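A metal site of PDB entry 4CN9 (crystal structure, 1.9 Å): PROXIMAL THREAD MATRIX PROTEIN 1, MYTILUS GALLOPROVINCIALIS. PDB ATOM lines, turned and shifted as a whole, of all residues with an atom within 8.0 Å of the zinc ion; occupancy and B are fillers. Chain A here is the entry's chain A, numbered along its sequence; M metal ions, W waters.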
ATOM      1  N   ASP A  61      15.615 -16.854  21.783  1.00  0.00           N
ATOM      2  CA  ASP A  61      15.660 -17.316  23.185  1.00  0.00           C
ATOM      3  C   ASP A  61      15.767 -16.097  24.115  1.00  0.00           C
ATOM      4  O   ASP A  61      16.718 -15.311  23.969  1.00  0.00           O
ATOM      5  CB  ASP A  61      16.861 -18.246  23.340  1.00  0.00           C
ATOM      6  CG  ASP A  61      17.004 -18.893  24.739  1.00  0.00           C
ATOM      7  OD1 ASP A  61      16.663 -18.283  25.774  1.00  0.00           O
ATOM      8  OD2 ASP A  61      17.524 -20.022  24.781  1.00  0.00           O
ATOM      9  N   ASP A  62      14.796 -15.897  25.013  1.00  0.00           N
ATOM     10  CA  ASP A  62      14.925 -14.820  26.017  1.00  0.00           C
ATOM     11  C   ASP A  62      14.944 -15.352  27.450  1.00  0.00           C
ATOM     12  O   ASP A  62      14.421 -14.726  28.362  1.00  0.00           O
ATOM     13  CB  ASP A  62      13.913 -13.665  25.814  1.00  0.00           C
ATOM     14  CG  ASP A  62      12.447 -14.062  26.034  1.00  0.00           C
ATOM     15  OD1 ASP A  62      12.112 -15.263  26.171  1.00  0.00           O
ATOM     16  OD2 ASP A  62      11.608 -13.134  26.068  1.00  0.00           O
ATOM     17  N   SER A  63      15.604 -16.498  27.629  1.00  0.00           N
ATOM     18  CA  SER A  63      15.808 -17.089  28.957  1.00  0.00           C
ATOM     19  C   SER A  63      16.803 -16.291  29.801  1.00  0.00           C
ATOM     20  O   SER A  63      17.711 -15.641  29.276  1.00  0.00           O
ATOM     21  CB  SER A  63      16.300 -18.545  28.832  1.00  0.00           C
ATOM     22  OG  SER A  63      17.586 -18.641  28.213  1.00  0.00           O
ATOM     23  N   SER A  64      16.653 -16.392  31.121  1.00  0.00           N
ATOM     24  CA  SER A  64      17.458 -15.616  32.068  1.00  0.00           C
ATOM     25  C   SER A  64      18.934 -16.001  32.021  1.00  0.00           C
ATOM     26  O   SER A  64      19.788 -15.188  32.357  1.00  0.00           O
ATOM     27  CB  SER A  64      16.923 -15.810  33.491  1.00  0.00           C
ATOM     28  OG  SER A  64      16.991 -17.179  33.858  1.00  0.00           O
ATOM     29  N   SER A  65      19.238 -17.216  31.597  1.00  0.00           N
ATOM     30  CA  SER A  65      20.635 -17.658  31.450  1.00  0.00           C
ATOM     31  C   SER A  65      21.486 -16.681  30.630  1.00  0.00           C
ATOM     32  O   SER A  65      22.672 -16.501  30.909  1.00  0.00           O
ATOM     33  CB  SER A  65      20.670 -19.036  30.777  1.00  0.00           C
ATOM     34  OG  SER A  65      20.225 -18.939  29.428  1.00  0.00           O
ATOM     35  N   ILE A  66      20.874 -16.040  29.648  1.00  0.00           N
ATOM     36  CA  ILE A  66      21.580 -15.147  28.753  1.00  0.00           C
ATOM     37  C   ILE A  66      22.020 -13.878  29.457  1.00  0.00           C
ATOM     38  O   ILE A  66      23.140 -13.405  29.252  1.00  0.00           O
ATOM     39  CB  ILE A  66      20.698 -14.786  27.542  1.00  0.00           C
ATOM     40  CG1 ILE A  66      20.362 -16.066  26.774  1.00  0.00           C
ATOM     41  CG2 ILE A  66      21.407 -13.748  26.649  1.00  0.00           C
ATOM     42  CD1 ILE A  66      19.393 -15.890  25.643  1.00  0.00           C
ATOM     43  N   GLN A  67      21.131 -13.325  30.286  1.00  0.00           N
ATOM     44  CA  GLN A  67      21.407 -12.093  30.995  1.00  0.00           C
ATOM     45  C   GLN A  67      22.422 -12.354  32.112  1.00  0.00           C
ATOM     46  O   GLN A  67      23.316 -11.547  32.323  1.00  0.00           O
ATOM     47  CB  GLN A  67      20.098 -11.488  31.542  1.00  0.00           C
ATOM     48  CG  GLN A  67      20.266 -10.211  32.379  1.00  0.00           C
ATOM     49  CD  GLN A  67      20.743  -9.022  31.561  1.00  0.00           C
ATOM     50  OE1 GLN A  67      20.489  -8.915  30.360  1.00  0.00           O
ATOM     51  NE2 GLN A  67      21.441  -8.105  32.233  1.00  0.00           N
ATOM     52  N   TYR A  74      22.249  -9.784  25.000  1.00  0.00           N
ATOM     53  CA  TYR A  74      21.034  -9.502  24.232  1.00  0.00           C
ATOM     54  C   TYR A  74      21.290  -8.494  23.119  1.00  0.00           C
ATOM     55  O   TYR A  74      20.728  -8.608  22.033  1.00  0.00           O
ATOM     56  CB  TYR A  74      19.896  -8.992  25.125  1.00  0.00           C
ATOM     57  CG  TYR A  74      19.172 -10.081  25.880  1.00  0.00           C
ATOM     58  CD1 TYR A  74      18.680 -11.215  25.220  1.00  0.00           C
ATOM     59  CD2 TYR A  74      18.976  -9.978  27.258  1.00  0.00           C
ATOM     60  CE1 TYR A  74      18.011 -12.208  25.923  1.00  0.00           C
ATOM     61  CE2 TYR A  74      18.314 -10.983  27.964  1.00  0.00           C
ATOM     62  CZ  TYR A  74      17.835 -12.099  27.287  1.00  0.00           C
ATOM     63  OH  TYR A  74      17.161 -13.089  27.978  1.00  0.00           O
ATOM     64  N   PHE A 106      11.004 -16.610  22.993  1.00  0.00           N
ATOM     65  CA  PHE A 106      10.593 -17.813  23.698  1.00  0.00           C
ATOM     66  C   PHE A 106      11.536 -18.141  24.848  1.00  0.00           C
ATOM     67  O   PHE A 106      12.765 -17.974  24.731  1.00  0.00           O
ATOM     68  CB  PHE A 106      10.508 -19.013  22.734  1.00  0.00           C
ATOM     69  CG  PHE A 106      11.845 -19.674  22.471  1.00  0.00           C
ATOM     70  CD1 PHE A 106      12.697 -19.187  21.472  1.00  0.00           C
ATOM     71  CD2 PHE A 106      12.266 -20.746  23.235  1.00  0.00           C
ATOM     72  CE1 PHE A 106      13.937 -19.775  21.255  1.00  0.00           C
ATOM     73  CE2 PHE A 106      13.511 -21.337  23.031  1.00  0.00           C
ATOM     74  CZ  PHE A 106      14.339 -20.853  22.032  1.00  0.00           C
ATOM     75  N   SER A 107      10.953 -18.564  25.965  1.00  0.00           N
ATOM     76  CA  SER A 107      11.687 -19.184  27.076  1.00  0.00           C
ATOM     77  C   SER A 107      10.641 -19.842  27.967  1.00  0.00           C
ATOM     78  O   SER A 107      10.302 -21.022  27.787  1.00  0.00           O
ATOM     79  CB  SER A 107      12.585 -18.191  27.847  1.00  0.00           C
ATOM     80  OG  SER A 107      11.936 -16.985  28.218  1.00  0.00           O
ATOM     81  N   GLY A 137      12.925 -15.540  30.986  1.00  0.00           N
ATOM     82  CA  GLY A 137      12.156 -16.651  31.536  1.00  0.00           C
ATOM     83  C   GLY A 137      13.034 -17.692  32.193  1.00  0.00           C
ATOM     84  O   GLY A 137      14.227 -17.835  31.883  1.00  0.00           O
ATOM     85  N   GLY A 138      12.432 -18.450  33.113  1.00  0.00           N
ATOM     86  CA  GLY A 138      13.144 -19.450  33.895  1.00  0.00           C
ATOM     87  C   GLY A 138      13.125 -20.845  33.308  1.00  0.00           C
ATOM     88  O   GLY A 138      13.559 -21.789  33.958  1.00  0.00           O
ATOM     89  N   GLN A 139      12.604 -20.974  32.087  1.00  0.00           N
ATOM     90  CA  GLN A 139      12.477 -22.237  31.377  1.00  0.00           C
ATOM     91  C   GLN A 139      12.879 -22.011  29.917  1.00  0.00           C
ATOM     92  O   GLN A 139      12.918 -20.871  29.464  1.00  0.00           O
ATOM     93  CB  GLN A 139      11.024 -22.710  31.350  1.00  0.00           C
ATOM     94  CG  GLN A 139      10.360 -22.928  32.684  1.00  0.00           C
ATOM     95  CD  GLN A 139       8.943 -23.466  32.520  1.00  0.00           C
ATOM     96  OE1 GLN A 139       8.328 -23.337  31.456  1.00  0.00           O
ATOM     97  NE2 GLN A 139       8.412 -24.074  33.581  1.00  0.00           N
ATOM     98  N   THR A 140      13.104 -23.088  29.177  1.00  0.00           N
ATOM     99  CA  THR A 140      13.381 -22.996  27.739  1.00  0.00           C
ATOM    100  C   THR A 140      12.457 -23.927  26.946  1.00  0.00           C
ATOM    101  O   THR A 140      12.704 -25.127  26.847  1.00  0.00           O
ATOM    102  CB  THR A 140      14.856 -23.336  27.441  1.00  0.00           C
ATOM    103  OG1 THR A 140      15.708 -22.452  28.180  1.00  0.00           O
ATOM    104  CG2 THR A 140      15.184 -23.200  25.948  1.00  0.00           C
ATOM    105  N   THR A 173      19.335 -20.293  20.332  1.00  0.00           N
ATOM    106  CA  THR A 173      19.168 -20.683  21.729  1.00  0.00           C
ATOM    107  C   THR A 173      20.486 -20.938  22.465  1.00  0.00           C
ATOM    108  O   THR A 173      21.486 -21.299  21.851  1.00  0.00           O
ATOM    109  CB  THR A 173      18.264 -21.927  21.826  1.00  0.00           C
ATOM    110  OG1 THR A 173      17.993 -22.233  23.211  1.00  0.00           O
ATOM    111  CG2 THR A 173      18.893 -23.107  21.152  1.00  0.00           C
ATOM    112  N   ASP A 174      20.474 -20.711  23.782  1.00  0.00           N
ATOM    113  CA  ASP A 174      21.624 -21.045  24.608  1.00  0.00           C
ATOM    114  C   ASP A 174      21.287 -22.168  25.575  1.00  0.00           C
ATOM    115  O   ASP A 174      21.997 -22.387  26.560  1.00  0.00           O
ATOM    116  CB  ASP A 174      22.119 -19.810  25.369  1.00  0.00           C
ATOM    117  CG  ASP A 174      21.335 -19.537  26.655  1.00  0.00           C
ATOM    118  OD1 ASP A 174      20.111 -19.847  26.730  1.00  0.00           O
ATOM    119  OD2 ASP A 174      21.966 -19.004  27.600  1.00  0.00           O
ATOM    120  N   GLY A 175      20.225 -22.905  25.280  1.00  0.00           N
ATOM    121  CA  GLY A 175      19.746 -23.902  26.230  1.00  0.00           C
ATOM    122  C   GLY A 175      19.177 -25.154  25.600  1.00  0.00           C
ATOM    123  O   GLY A 175      19.115 -25.288  24.372  1.00  0.00           O
ATOM    124  N   LYS A 176      18.747 -26.077  26.441  1.00  0.00           N
ATOM    125  CA  LYS A 176      18.080 -27.268  25.955  1.00  0.00           C
ATOM    126  C   LYS A 176      16.619 -27.178  26.365  1.00  0.00           C
ATOM    127  O   LYS A 176      16.301 -26.562  27.378  1.00  0.00           O
ATOM    128  CB  LYS A 176      18.729 -28.535  26.511  1.00  0.00           C
ATOM    129  CG  LYS A 176      18.578 -28.722  28.003  1.00  0.00           C
ATOM    130  CD  LYS A 176      19.167 -30.059  28.434  1.00  0.00           C
ATOM    131  CE  LYS A 176      19.397 -30.094  29.931  1.00  0.00           C
ATOM    132  NZ  LYS A 176      20.050 -31.366  30.368  1.00  0.00           N
ATOM    133  N   ASN A 178      13.380 -27.820  28.057  1.00  0.00           N
ATOM    134  CA  ASN A 178      13.143 -28.499  29.333  1.00  0.00           C
ATOM    135  C   ASN A 178      11.730 -28.335  29.875  1.00  0.00           C
ATOM    136  O   ASN A 178      11.490 -28.590  31.044  1.00  0.00           O
ATOM    137  CB  ASN A 178      14.147 -28.058  30.397  1.00  0.00           C
ATOM    138  CG  ASN A 178      14.053 -26.563  30.718  1.00  0.00           C
ATOM    139  OD1 ASN A 178      13.251 -25.850  30.156  1.00  0.00           O
ATOM    140  ND2 ASN A 178      14.885 -26.106  31.641  1.00  0.00           N
ATOM    141  N   ILE A 202      24.310 -21.462  21.030  1.00  0.00           N
ATOM    142  CA  ILE A 202      25.332 -20.619  21.636  1.00  0.00           C
ATOM    143  C   ILE A 202      25.714 -21.122  23.020  1.00  0.00           C
ATOM    144  O   ILE A 202      24.860 -21.388  23.856  1.00  0.00           O
ATOM    145  CB  ILE A 202      24.838 -19.179  21.728  1.00  0.00           C
ATOM    146  CG1 ILE A 202      24.457 -18.676  20.343  1.00  0.00           C
ATOM    147  CG2 ILE A 202      25.938 -18.280  22.302  1.00  0.00           C
ATOM    148  CD1 ILE A 202      23.124 -17.991  20.270  1.00  0.00           C
ATOM    149  N   GLY A 205      25.193 -24.774  26.918  1.00  0.00           N
ATOM    150  CA  GLY A 205      23.940 -25.240  27.513  1.00  0.00           C
ATOM    151  C   GLY A 205      22.948 -25.922  26.573  1.00  0.00           C
ATOM    152  O   GLY A 205      22.052 -26.628  27.027  1.00  0.00           O
ATOM    153  N   PHE A 206      23.106 -25.709  25.269  1.00  0.00           N
ATOM    154  CA  PHE A 206      22.261 -26.385  24.284  1.00  0.00           C
ATOM    155  C   PHE A 206      22.779 -27.811  24.039  1.00  0.00           C
ATOM    156  O   PHE A 206      23.927 -28.120  24.363  1.00  0.00           O
ATOM    157  CB  PHE A 206      22.230 -25.572  22.968  1.00  0.00           C
ATOM    158  CG  PHE A 206      23.493 -25.697  22.143  1.00  0.00           C
ATOM    159  CD1 PHE A 206      23.628 -26.712  21.211  1.00  0.00           C
ATOM    160  CD2 PHE A 206      24.543 -24.802  22.303  1.00  0.00           C
ATOM    161  CE1 PHE A 206      24.776 -26.836  20.467  1.00  0.00           C
ATOM    162  CE2 PHE A 206      25.706 -24.919  21.555  1.00  0.00           C
ATOM    163  CZ  PHE A 206      25.824 -25.932  20.638  1.00  0.00           C
ATOM    164  N   PHE A 227      28.311 -15.343  22.555  1.00  0.00           N
ATOM    165  CA  PHE A 227      27.487 -14.384  21.844  1.00  0.00           C
ATOM    166  C   PHE A 227      28.371 -13.402  21.081  1.00  0.00           C
ATOM    167  O   PHE A 227      27.962 -12.818  20.090  1.00  0.00           O
ATOM    168  CB  PHE A 227      26.572 -13.645  22.826  1.00  0.00           C
ATOM    169  CG  PHE A 227      25.557 -14.534  23.488  1.00  0.00           C
ATOM    170  CD1 PHE A 227      25.858 -15.206  24.661  1.00  0.00           C
ATOM    171  CD2 PHE A 227      24.306 -14.720  22.930  1.00  0.00           C
ATOM    172  CE1 PHE A 227      24.923 -16.027  25.272  1.00  0.00           C
ATOM    173  CE2 PHE A 227      23.364 -15.548  23.527  1.00  0.00           C
ATOM    174  CZ  PHE A 227      23.674 -16.201  24.693  1.00  0.00           C
HETATM  175 ZN    ZN M   1      18.994 -20.264  28.476  1.00  0.00          ZN
HETATM  176  O   HOH W   1      17.838 -21.324  27.111  1.00  0.00           O
HETATM  177  O   HOH W   2      20.292 -21.876  28.897  1.00  0.00           O
HETATM  178  O   HOH W   3      17.975 -20.951  30.152  1.00  0.00           O
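Water W1 lies within hydrogen-bond range of the side-chain hydroxyl (OG1) of Thr 140, the side-chain carboxylate (OD2) of Asp 61 and the backbone NH (N) of Gly 175.
The zinc ion is bound by the side-chain hydroxyl (OG) of Ser 65, water W1, water W3, water W2, the side-chain carboxylate (OD1) of Asp 174 and the side-chain hydroxyl (OG) of Ser 63.
Asp 61 touches the zinc ion.
Thr 140 touches the zinc ion.
Of the 23 residues printed, 5 come within 4 Å of the zinc ion.
N of Ser 63 sits at hydrogen-bond distance from OD1 of Asp 61 (2.8 Å).
The backbone NH of Asp 174 sits at hydrogen-bond distance from the side-chain carboxylate of Asp 61 (3.2 Å).
The backbone carbonyl oxygen of Ser 63 lies within hydrogen-bond range of the side-chain hydroxyl of Tyr 74 (2.9 Å).
The side-chain carboxylate (OD2) of Asp 61 sits at hydrogen-bond distance from the side-chain hydroxyl (OG1) of Thr 173.
The backbone NH (N) of Thr 140 lies within hydrogen-bond range of the side-chain amide oxygen (OD1) of Asn 178 (2.9 Å).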
